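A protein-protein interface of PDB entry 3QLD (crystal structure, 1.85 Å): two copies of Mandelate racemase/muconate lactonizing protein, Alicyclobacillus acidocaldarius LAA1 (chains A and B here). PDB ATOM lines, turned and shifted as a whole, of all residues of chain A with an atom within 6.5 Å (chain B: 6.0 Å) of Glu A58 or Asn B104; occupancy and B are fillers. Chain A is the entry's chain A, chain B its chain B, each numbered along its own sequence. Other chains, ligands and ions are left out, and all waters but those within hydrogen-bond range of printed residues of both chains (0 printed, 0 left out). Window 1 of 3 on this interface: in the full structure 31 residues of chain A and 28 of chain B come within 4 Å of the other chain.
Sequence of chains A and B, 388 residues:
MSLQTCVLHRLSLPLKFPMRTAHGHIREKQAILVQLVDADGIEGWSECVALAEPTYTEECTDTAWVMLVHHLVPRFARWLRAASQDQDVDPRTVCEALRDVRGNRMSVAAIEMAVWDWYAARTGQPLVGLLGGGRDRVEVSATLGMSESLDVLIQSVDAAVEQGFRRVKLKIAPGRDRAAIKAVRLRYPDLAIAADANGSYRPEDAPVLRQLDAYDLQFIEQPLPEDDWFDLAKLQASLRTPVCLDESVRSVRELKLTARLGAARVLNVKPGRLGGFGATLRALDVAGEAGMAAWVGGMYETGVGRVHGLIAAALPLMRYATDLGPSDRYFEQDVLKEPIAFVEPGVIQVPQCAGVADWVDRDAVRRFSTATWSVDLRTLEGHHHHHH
The side-chain amide nitrogen (ND2) of Asn B104 is in hydrogen-bond range of the backbone carbonyl oxygen (O) of Glu A58. The side-chain amide nitrogen of Asn A104 sits at hydrogen-bond distance from the backbone carbonyl oxygen of Glu B58 (3.0 Å). NH2 of Arg B102 lies within hydrogen-bond range of O of Thr A55, at 3.3 Å. The backbone carbonyl oxygen (O) of Tyr A56 lies within hydrogen-bond range of the guanidinium group (NH2) of Arg B102 (3.0 Å). The backbone carbonyl oxygen of Pro A54 is in hydrogen-bond range of the backbone NH of Arg B102, 2.8 Å away.
The side-chain carboxylate (OE1) of Glu A58 lies within salt-bridge range of the guanidinium group (NE) of Arg A250. OG1 of Thr A63 sits at hydrogen-bond distance from O of Cys A60, at 3.2 Å. The backbone NH (N) of Leu B72 lies within hydrogen-bond range of the backbone carbonyl oxygen (O) of Met B67. The backbone carbonyl oxygen (O) of Arg B102 sits at hydrogen-bond distance from the side-chain amide nitrogen (ND2) of Asn B104 (3.0 Å). The side-chain hydroxyl of Thr A57 lies close to the side-chain sulfur of Met A106 (3.8 Å).
Among the printed residues, pairs that only touch across the chains: Glu A58 with Arg B102 (3.4 Å), Thr A63 with Thr B63 (3.4 Å), Pro A54 with Val B101 (3.5 Å), Thr A57 with Arg B102 (3.6 Å), Thr A63 with Met B67 (3.7 Å), Cys A60 with Met B67 (3.7 Å), Pro A54 with Asn B104 (3.9 Å) and Pro A54 with Met B67 (3.9 Å).
Of the printed residues of chain B, Glu A58 touches Arg B102 and Asn B104. Asn B104 touches just these residues of chain A: Pro A54 (3.9 Å) and Glu A58 (3.0 Å). Printed residues of chain A within 4 Å of Thr B63: Thr A63. Of the printed residues of chain B, Asn A104 touches Glu B58. Of the printed residues of chain B, Tyr A56 touches Arg B102 (3.0 Å). The nearest printed residue of chain B that does not touch Glu A58 is Gly B103 (4.004 Å).
Printed residues of chain B that touch a printed residue of chain A: Glu B58, Thr B63, Met B67, Val B101, Arg B102 and Asn B104. Of the 13 printed residues of chain A, 8 touch a printed residue of chain B. Hydrophobic or aromatic side chains of chain A within 4 Å of the printed part of chain B: Pro A54.
Glu A58 touches Asn B104, and with the chains exchanged Asn A104 touches Glu B58. Thr B63 touches its own counterpart, Thr A63. Positions printed for both chains: 58, 59, 63, 103, 104, 105 and 106. Of the 13 pairs that touch across the chains among the printed residues, 3 have their exchanged pair printed and touching as well.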
ATOM      1  N   PRO A  54       4.016 -12.608  10.419  1.00  0.00           N
ATOM      2  CA  PRO A  54       2.601 -12.709  10.196  1.00  0.00           C
ATOM      3  C   PRO A  54       1.842 -11.444  10.539  1.00  0.00           C
ATOM      4  O   PRO A  54       0.876 -11.492  11.287  1.00  0.00           O
ATOM      5  CB  PRO A  54       2.183 -13.913  11.075  1.00  0.00           C
ATOM      6  CG  PRO A  54       3.019 -13.678  12.344  1.00  0.00           C
ATOM      7  CD  PRO A  54       4.402 -13.169  11.732  1.00  0.00           C
ATOM      8  N   THR A  55       2.276 -10.339   9.947  1.00  0.00           N
ATOM      9  CA  THR A  55       1.710  -9.000  10.252  1.00  0.00           C
ATOM     10  C   THR A  55       0.823  -8.463   9.132  1.00  0.00           C
ATOM     11  O   THR A  55       0.020  -7.538   9.332  1.00  0.00           O
ATOM     12  CB  THR A  55       2.782  -7.965  10.497  1.00  0.00           C
ATOM     13  OG1 THR A  55       3.638  -7.911   9.370  1.00  0.00           O
ATOM     14  CG2 THR A  55       3.578  -8.240  11.795  1.00  0.00           C
ATOM     15  N   TYR A  56       0.919  -9.042   7.956  1.00  0.00           N
ATOM     16  CA  TYR A  56      -0.046  -8.735   6.896  1.00  0.00           C
ATOM     17  C   TYR A  56      -1.115  -9.806   6.715  1.00  0.00           C
ATOM     18  O   TYR A  56      -2.319  -9.507   6.703  1.00  0.00           O
ATOM     19  CB  TYR A  56       0.752  -8.468   5.620  1.00  0.00           C
ATOM     20  CG  TYR A  56       0.017  -8.576   4.289  1.00  0.00           C
ATOM     21  CD1 TYR A  56      -0.951  -7.631   3.880  1.00  0.00           C
ATOM     22  CD2 TYR A  56       0.328  -9.577   3.407  1.00  0.00           C
ATOM     23  CE1 TYR A  56      -1.611  -7.719   2.626  1.00  0.00           C
ATOM     24  CE2 TYR A  56      -0.353  -9.688   2.150  1.00  0.00           C
ATOM     25  CZ  TYR A  56      -1.303  -8.738   1.767  1.00  0.00           C
ATOM     26  OH  TYR A  56      -1.903  -8.854   0.509  1.00  0.00           O
ATOM     27  N   THR A  57      -0.715 -11.080   6.613  1.00  0.00           N
ATOM     28  CA  THR A  57      -1.652 -12.155   6.822  1.00  0.00           C
ATOM     29  C   THR A  57      -1.071 -13.167   7.838  1.00  0.00           C
ATOM     30  O   THR A  57      -0.019 -12.931   8.385  1.00  0.00           O
ATOM     31  CB  THR A  57      -2.044 -12.920   5.548  1.00  0.00           C
ATOM     32  OG1 THR A  57      -0.909 -13.651   5.084  1.00  0.00           O
ATOM     33  CG2 THR A  57      -2.534 -11.938   4.406  1.00  0.00           C
ATOM     34  N   GLU A  58      -1.769 -14.283   8.017  1.00  0.00           N
ATOM     35  CA  GLU A  58      -1.436 -15.247   9.094  1.00  0.00           C
ATOM     36  C   GLU A  58      -0.260 -16.137   8.683  1.00  0.00           C
ATOM     37  O   GLU A  58       0.352 -16.764   9.543  1.00  0.00           O
ATOM     38  CB  GLU A  58      -2.651 -16.087   9.485  1.00  0.00           C
ATOM     39  CG  GLU A  58      -3.108 -17.130   8.414  1.00  0.00           C
ATOM     40  CD  GLU A  58      -3.822 -16.518   7.192  1.00  0.00           C
ATOM     41  OE1 GLU A  58      -4.230 -15.313   7.211  1.00  0.00           O
ATOM     42  OE2 GLU A  58      -3.995 -17.280   6.215  1.00  0.00           O
ATOM     43  N   GLU A  59       0.060 -16.162   7.382  1.00  0.00           N
ATOM     44  CA  GLU A  59       1.215 -16.971   6.876  1.00  0.00           C
ATOM     45  C   GLU A  59       2.537 -16.202   6.989  1.00  0.00           C
ATOM     46  O   GLU A  59       2.590 -14.988   6.820  1.00  0.00           O
ATOM     47  CB  GLU A  59       0.906 -17.470   5.408  1.00  0.00           C
ATOM     48  CG  GLU A  59      -0.351 -18.424   5.334  1.00  0.00           C
ATOM     49  CD  GLU A  59      -0.557 -18.852   3.876  1.00  0.00           C
ATOM     50  OE1 GLU A  59       0.157 -19.792   3.481  1.00  0.00           O
ATOM     51  OE2 GLU A  59      -1.304 -18.182   3.151  1.00  0.00           O
ATOM     52  N   CYS A  60       3.626 -16.884   7.328  1.00  0.00           N
ATOM     53  CA  CYS A  60       4.885 -16.230   7.251  1.00  0.00           C
ATOM     54  C   CYS A  60       5.865 -17.259   6.681  1.00  0.00           C
ATOM     55  O   CYS A  60       5.511 -18.457   6.481  1.00  0.00           O
ATOM     56  CB  CYS A  60       5.305 -15.665   8.635  1.00  0.00           C
ATOM     57  SG  CYS A  60       5.645 -17.047   9.902  1.00  0.00           S
ATOM     58  N   THR A  63       6.348 -20.646   8.644  1.00  0.00           N
ATOM     59  CA  THR A  63       5.235 -21.552   8.667  1.00  0.00           C
ATOM     60  C   THR A  63       4.937 -22.089   7.257  1.00  0.00           C
ATOM     61  O   THR A  63       4.601 -23.267   7.127  1.00  0.00           O
ATOM     62  CB  THR A  63       3.962 -20.967   9.304  1.00  0.00           C
ATOM     63  OG1 THR A  63       3.582 -19.777   8.616  1.00  0.00           O
ATOM     64  CG2 THR A  63       4.234 -20.626  10.833  1.00  0.00           C
ATOM     65  N   GLY A 103      -7.263 -22.930   4.598  1.00  0.00           N
ATOM     66  CA  GLY A 103      -6.436 -21.733   4.501  1.00  0.00           C
ATOM     67  C   GLY A 103      -5.123 -22.037   3.820  1.00  0.00           C
ATOM     68  O   GLY A 103      -5.093 -22.832   2.818  1.00  0.00           O
ATOM     69  N   ASN A 104      -4.059 -21.454   4.362  1.00  0.00           N
ATOM     70  CA  ASN A 104      -2.664 -21.668   3.832  1.00  0.00           C
ATOM     71  C   ASN A 104      -2.587 -21.331   2.359  1.00  0.00           C
ATOM     72  O   ASN A 104      -1.923 -22.021   1.560  1.00  0.00           O
ATOM     73  CB  ASN A 104      -2.234 -23.112   4.075  1.00  0.00           C
ATOM     74  CG  ASN A 104      -1.975 -23.361   5.587  1.00  0.00           C
ATOM     75  OD1 ASN A 104      -0.906 -22.973   6.099  1.00  0.00           O
ATOM     76  ND2 ASN A 104      -2.935 -23.979   6.275  1.00  0.00           N
ATOM     77  N   ARG A 105      -3.308 -20.275   1.979  1.00  0.00           N
ATOM     78  CA  ARG A 105      -3.459 -20.022   0.543  1.00  0.00           C
ATOM     79  C   ARG A 105      -2.178 -19.607  -0.169  1.00  0.00           C
ATOM     80  O   ARG A 105      -2.040 -19.914  -1.360  1.00  0.00           O
ATOM     81  CB  ARG A 105      -4.567 -19.024   0.285  1.00  0.00           C
ATOM     82  CG  ARG A 105      -5.907 -19.712   0.479  1.00  0.00           C
ATOM     83  CD  ARG A 105      -7.054 -18.704   0.167  1.00  0.00           C
ATOM     84  NE  ARG A 105      -8.383 -19.325   0.346  1.00  0.00           N
ATOM     85  CZ  ARG A 105      -9.203 -19.677  -0.653  1.00  0.00           C
ATOM     86  NH1 ARG A 105      -8.900 -19.419  -1.942  1.00  0.00           N
ATOM     87  NH2 ARG A 105     -10.368 -20.255  -0.358  1.00  0.00           N
ATOM     88  N   MET A 106      -1.251 -18.932   0.524  1.00  0.00           N
ATOM     89  CA  MET A 106       0.007 -18.574  -0.137  1.00  0.00           C
ATOM     90  C   MET A 106       0.904 -19.797  -0.407  1.00  0.00           C
ATOM     91  O   MET A 106       1.613 -19.845  -1.445  1.00  0.00           O
ATOM     92  CB  MET A 106       0.760 -17.485   0.646  1.00  0.00           C
ATOM     93  CG  MET A 106      -0.002 -16.148   0.691  1.00  0.00           C
ATOM     94  SD  MET A 106       0.823 -15.043   2.053  1.00  0.00           S
ATOM     95  CE  MET A 106      -0.233 -13.430   1.853  1.00  0.00           C
ATOM     96  N   ARG A 250      -9.384 -12.716   1.366  1.00  0.00           N
ATOM     97  CA  ARG A 250      -8.425 -13.823   1.215  1.00  0.00           C
ATOM     98  C   ARG A 250      -8.949 -14.960   0.359  1.00  0.00           C
ATOM     99  O   ARG A 250      -8.227 -15.931   0.161  1.00  0.00           O
ATOM    100  CB  ARG A 250      -8.093 -14.455   2.590  1.00  0.00           C
ATOM    101  CG  ARG A 250      -7.862 -13.540   3.772  1.00  0.00           C
ATOM    102  CD  ARG A 250      -6.427 -12.982   3.749  1.00  0.00           C
ATOM    103  NE  ARG A 250      -5.817 -12.504   5.019  1.00  0.00           N
ATOM    104  CZ  ARG A 250      -6.400 -11.959   6.111  1.00  0.00           C
ATOM    105  NH1 ARG A 250      -7.727 -11.793   6.230  1.00  0.00           N
ATOM    106  NH2 ARG A 250      -5.611 -11.556   7.128  1.00  0.00           N
ATOM    107  N   GLU B  58      -6.686 -23.867   9.763  1.00  0.00           N
ATOM    108  CA  GLU B  58      -5.457 -23.693   8.999  1.00  0.00           C
ATOM    109  C   GLU B  58      -4.191 -23.944   9.825  1.00  0.00           C
ATOM    110  O   GLU B  58      -3.153 -24.122   9.246  1.00  0.00           O
ATOM    111  CB  GLU B  58      -5.471 -22.278   8.398  1.00  0.00           C
ATOM    112  CG  GLU B  58      -5.201 -21.151   9.328  1.00  0.00           C
ATOM    113  CD  GLU B  58      -6.413 -20.800  10.254  1.00  0.00           C
ATOM    114  OE1 GLU B  58      -7.555 -21.285  10.006  1.00  0.00           O
ATOM    115  OE2 GLU B  58      -6.221 -19.994  11.212  1.00  0.00           O
ATOM    116  N   GLU B  59      -4.265 -23.928  11.178  1.00  0.00           N
ATOM    117  CA  GLU B  59      -3.048 -24.152  11.995  1.00  0.00           C
ATOM    118  C   GLU B  59      -2.868 -25.670  12.209  1.00  0.00           C
ATOM    119  O   GLU B  59      -3.857 -26.418  12.238  1.00  0.00           O
ATOM    120  CB  GLU B  59      -3.274 -23.501  13.404  1.00  0.00           C
ATOM    121  CG  GLU B  59      -3.451 -21.949  13.299  1.00  0.00           C
ATOM    122  CD  GLU B  59      -3.681 -21.352  14.692  1.00  0.00           C
ATOM    123  OE1 GLU B  59      -2.685 -21.161  15.419  1.00  0.00           O
ATOM    124  OE2 GLU B  59      -4.842 -21.080  14.982  1.00  0.00           O
ATOM    125  N   THR B  63       3.186 -26.049  12.216  1.00  0.00           N
ATOM    126  CA  THR B  63       3.301 -24.602  11.943  1.00  0.00           C
ATOM    127  C   THR B  63       3.139 -23.831  13.270  1.00  0.00           C
ATOM    128  O   THR B  63       3.749 -22.795  13.471  1.00  0.00           O
ATOM    129  CB  THR B  63       2.273 -24.060  10.911  1.00  0.00           C
ATOM    130  OG1 THR B  63       0.943 -24.330  11.373  1.00  0.00           O
ATOM    131  CG2 THR B  63       2.498 -24.673   9.553  1.00  0.00           C
ATOM    132  N   MET B  67       5.716 -21.011  14.757  1.00  0.00           N
ATOM    133  CA  MET B  67       5.064 -19.755  15.073  1.00  0.00           C
ATOM    134  C   MET B  67       5.388 -19.390  16.570  1.00  0.00           C
ATOM    135  O   MET B  67       5.732 -18.262  16.896  1.00  0.00           O
ATOM    136  CB  MET B  67       3.567 -19.888  14.758  1.00  0.00           C
ATOM    137  CG  MET B  67       2.709 -18.808  15.419  1.00  0.00           C
ATOM    138  SD  MET B  67       3.027 -17.014  14.510  1.00  0.00           S
ATOM    139  CE  MET B  67       3.254 -17.586  12.644  1.00  0.00           C
ATOM    140  N   LEU B  72       5.955 -15.805  18.326  1.00  0.00           N
ATOM    141  CA  LEU B  72       5.142 -15.354  19.447  1.00  0.00           C
ATOM    142  C   LEU B  72       5.915 -15.313  20.765  1.00  0.00           C
ATOM    143  O   LEU B  72       5.775 -14.361  21.539  1.00  0.00           O
ATOM    144  CB  LEU B  72       3.903 -16.285  19.587  1.00  0.00           C
ATOM    145  CG  LEU B  72       3.066 -16.393  18.314  1.00  0.00           C
ATOM    146  CD1 LEU B  72       1.781 -17.185  18.769  1.00  0.00           C
ATOM    147  CD2 LEU B  72       2.717 -14.999  17.736  1.00  0.00           C
ATOM    148  N   VAL B 101      -0.057  -9.569  15.263  1.00  0.00           N
ATOM    149  CA  VAL B 101      -0.090 -10.899  14.621  1.00  0.00           C
ATOM    150  C   VAL B 101      -1.458 -11.183  14.040  1.00  0.00           C
ATOM    151  O   VAL B 101      -2.471 -11.121  14.719  1.00  0.00           O
ATOM    152  CB  VAL B 101       0.278 -12.010  15.623  1.00  0.00           C
ATOM    153  CG1 VAL B 101       0.110 -13.394  14.998  1.00  0.00           C
ATOM    154  CG2 VAL B 101       1.765 -11.813  16.035  1.00  0.00           C
ATOM    155  N   ARG B 102      -1.495 -11.487  12.756  1.00  0.00           N
ATOM    156  CA  ARG B 102      -2.779 -11.898  12.181  1.00  0.00           C
ATOM    157  C   ARG B 102      -3.024 -13.400  12.387  1.00  0.00           C
ATOM    158  O   ARG B 102      -2.072 -14.174  12.256  1.00  0.00           O
ATOM    159  CB  ARG B 102      -2.774 -11.635  10.647  1.00  0.00           C
ATOM    160  CG  ARG B 102      -2.456 -10.134  10.365  1.00  0.00           C
ATOM    161  CD  ARG B 102      -3.722  -9.334  10.569  1.00  0.00           C
ATOM    162  NE  ARG B 102      -3.536  -7.887  10.717  1.00  0.00           N
ATOM    163  CZ  ARG B 102      -3.301  -6.973   9.755  1.00  0.00           C
ATOM    164  NH1 ARG B 102      -3.177  -5.682  10.115  1.00  0.00           N
ATOM    165  NH2 ARG B 102      -3.165  -7.291   8.459  1.00  0.00           N
ATOM    166  N   GLY B 103      -4.286 -13.784  12.607  1.00  0.00           N
ATOM    167  CA  GLY B 103      -4.714 -15.187  12.797  1.00  0.00           C
ATOM    168  C   GLY B 103      -3.785 -15.848  13.854  1.00  0.00           C
ATOM    169  O   GLY B 103      -3.464 -15.247  14.916  1.00  0.00           O
ATOM    170  N   ASN B 104      -3.398 -17.084  13.579  1.00  0.00           N
ATOM    171  CA  ASN B 104      -2.606 -17.874  14.506  1.00  0.00           C
ATOM    172  C   ASN B 104      -3.251 -17.890  15.862  1.00  0.00           C
ATOM    173  O   ASN B 104      -2.539 -17.873  16.884  1.00  0.00           O
ATOM    174  CB  ASN B 104      -1.209 -17.295  14.585  1.00  0.00           C
ATOM    175  CG  ASN B 104      -0.458 -17.583  13.303  1.00  0.00           C
ATOM    176  OD1 ASN B 104      -0.127 -18.765  13.021  1.00  0.00           O
ATOM    177  ND2 ASN B 104      -0.334 -16.560  12.449  1.00  0.00           N
ATOM    178  N   ARG B 105      -4.589 -17.958  15.902  1.00  0.00           N
ATOM    179  CA  ARG B 105      -5.193 -17.787  17.255  1.00  0.00           C
ATOM    180  C   ARG B 105      -4.945 -18.927  18.212  1.00  0.00           C
ATOM    181  O   ARG B 105      -4.892 -18.671  19.444  1.00  0.00           O
ATOM    182  CB  ARG B 105      -6.684 -17.586  17.117  1.00  0.00           C
ATOM    183  CG  ARG B 105      -6.999 -16.234  16.545  1.00  0.00           C
ATOM    184  CD  ARG B 105      -8.441 -15.848  16.849  1.00  0.00           C
ATOM    185  NE  ARG B 105      -8.886 -14.755  15.978  1.00  0.00           N
ATOM    186  CZ  ARG B 105      -9.125 -13.494  16.375  1.00  0.00           C
ATOM    187  NH1 ARG B 105      -8.996 -13.147  17.649  1.00  0.00           N
ATOM    188  NH2 ARG B 105      -9.521 -12.567  15.490  1.00  0.00           N
ATOM    189  N   MET B 106      -4.797 -20.159  17.698  1.00  0.00           N
ATOM    190  CA  MET B 106      -4.493 -21.291  18.627  1.00  0.00           C
ATOM    191  C   MET B 106      -3.088 -21.186  19.288  1.00  0.00           C
ATOM    192  O   MET B 106      -2.957 -21.616  20.461  1.00  0.00           O
ATOM    193  CB  MET B 106      -4.703 -22.704  17.950  1.00  0.00           C
ATOM    194  CG  MET B 106      -6.173 -22.919  17.622  1.00  0.00           C
ATOM    195  SD  MET B 106      -6.229 -24.433  16.325  1.00  0.00           S
ATOM    196  CE  MET B 106      -8.131 -24.312  16.155  1.00  0.00           C
ATOM    197  N   SER B 107      -2.080 -20.642  18.539  1.00  0.00           N
ATOM    198  CA  SER B 107      -0.690 -20.414  19.052  1.00  0.00           C
ATOM    199  C   SER B 107      -0.757 -19.259  20.083  1.00  0.00           C
ATOM    200  O   SER B 107      -0.270 -19.361  21.264  1.00  0.00           O
ATOM    201  CB  SER B 107       0.257 -20.122  17.830  1.00  0.00           C
ATOM    202  OG  SER B 107       0.395 -21.410  17.182  1.00  0.00           O
ATOM    203  N   VAL B 108      -1.497 -18.224  19.723  1.00  0.00           N
ATOM    204  CA  VAL B 108      -1.711 -17.097  20.640  1.00  0.00           C
ATOM    205  C   VAL B 108      -2.428 -17.559  21.901  1.00  0.00           C
ATOM    206  O   VAL B 108      -1.980 -17.223  23.012  1.00  0.00           O
ATOM    207  CB  VAL B 108      -2.556 -15.936  19.968  1.00  0.00           C
ATOM    208  CG1 VAL B 108      -3.131 -14.943  21.043  1.00  0.00           C
ATOM    209  CG2 VAL B 108      -1.703 -15.255  18.868  1.00  0.00           C
ATOM    210  N   ALA B 109      -3.459 -18.398  21.748  1.00  0.00           N
ATOM    211  CA  ALA B 109      -4.193 -18.913  22.915  1.00  0.00           C
ATOM    212  C   ALA B 109      -3.280 -19.695  23.863  1.00  0.00           C
ATOM    213  O   ALA B 109      -3.480 -19.608  25.090  1.00  0.00           O
ATOM    214  CB  ALA B 109      -5.351 -19.819  22.481  1.00  0.00           C
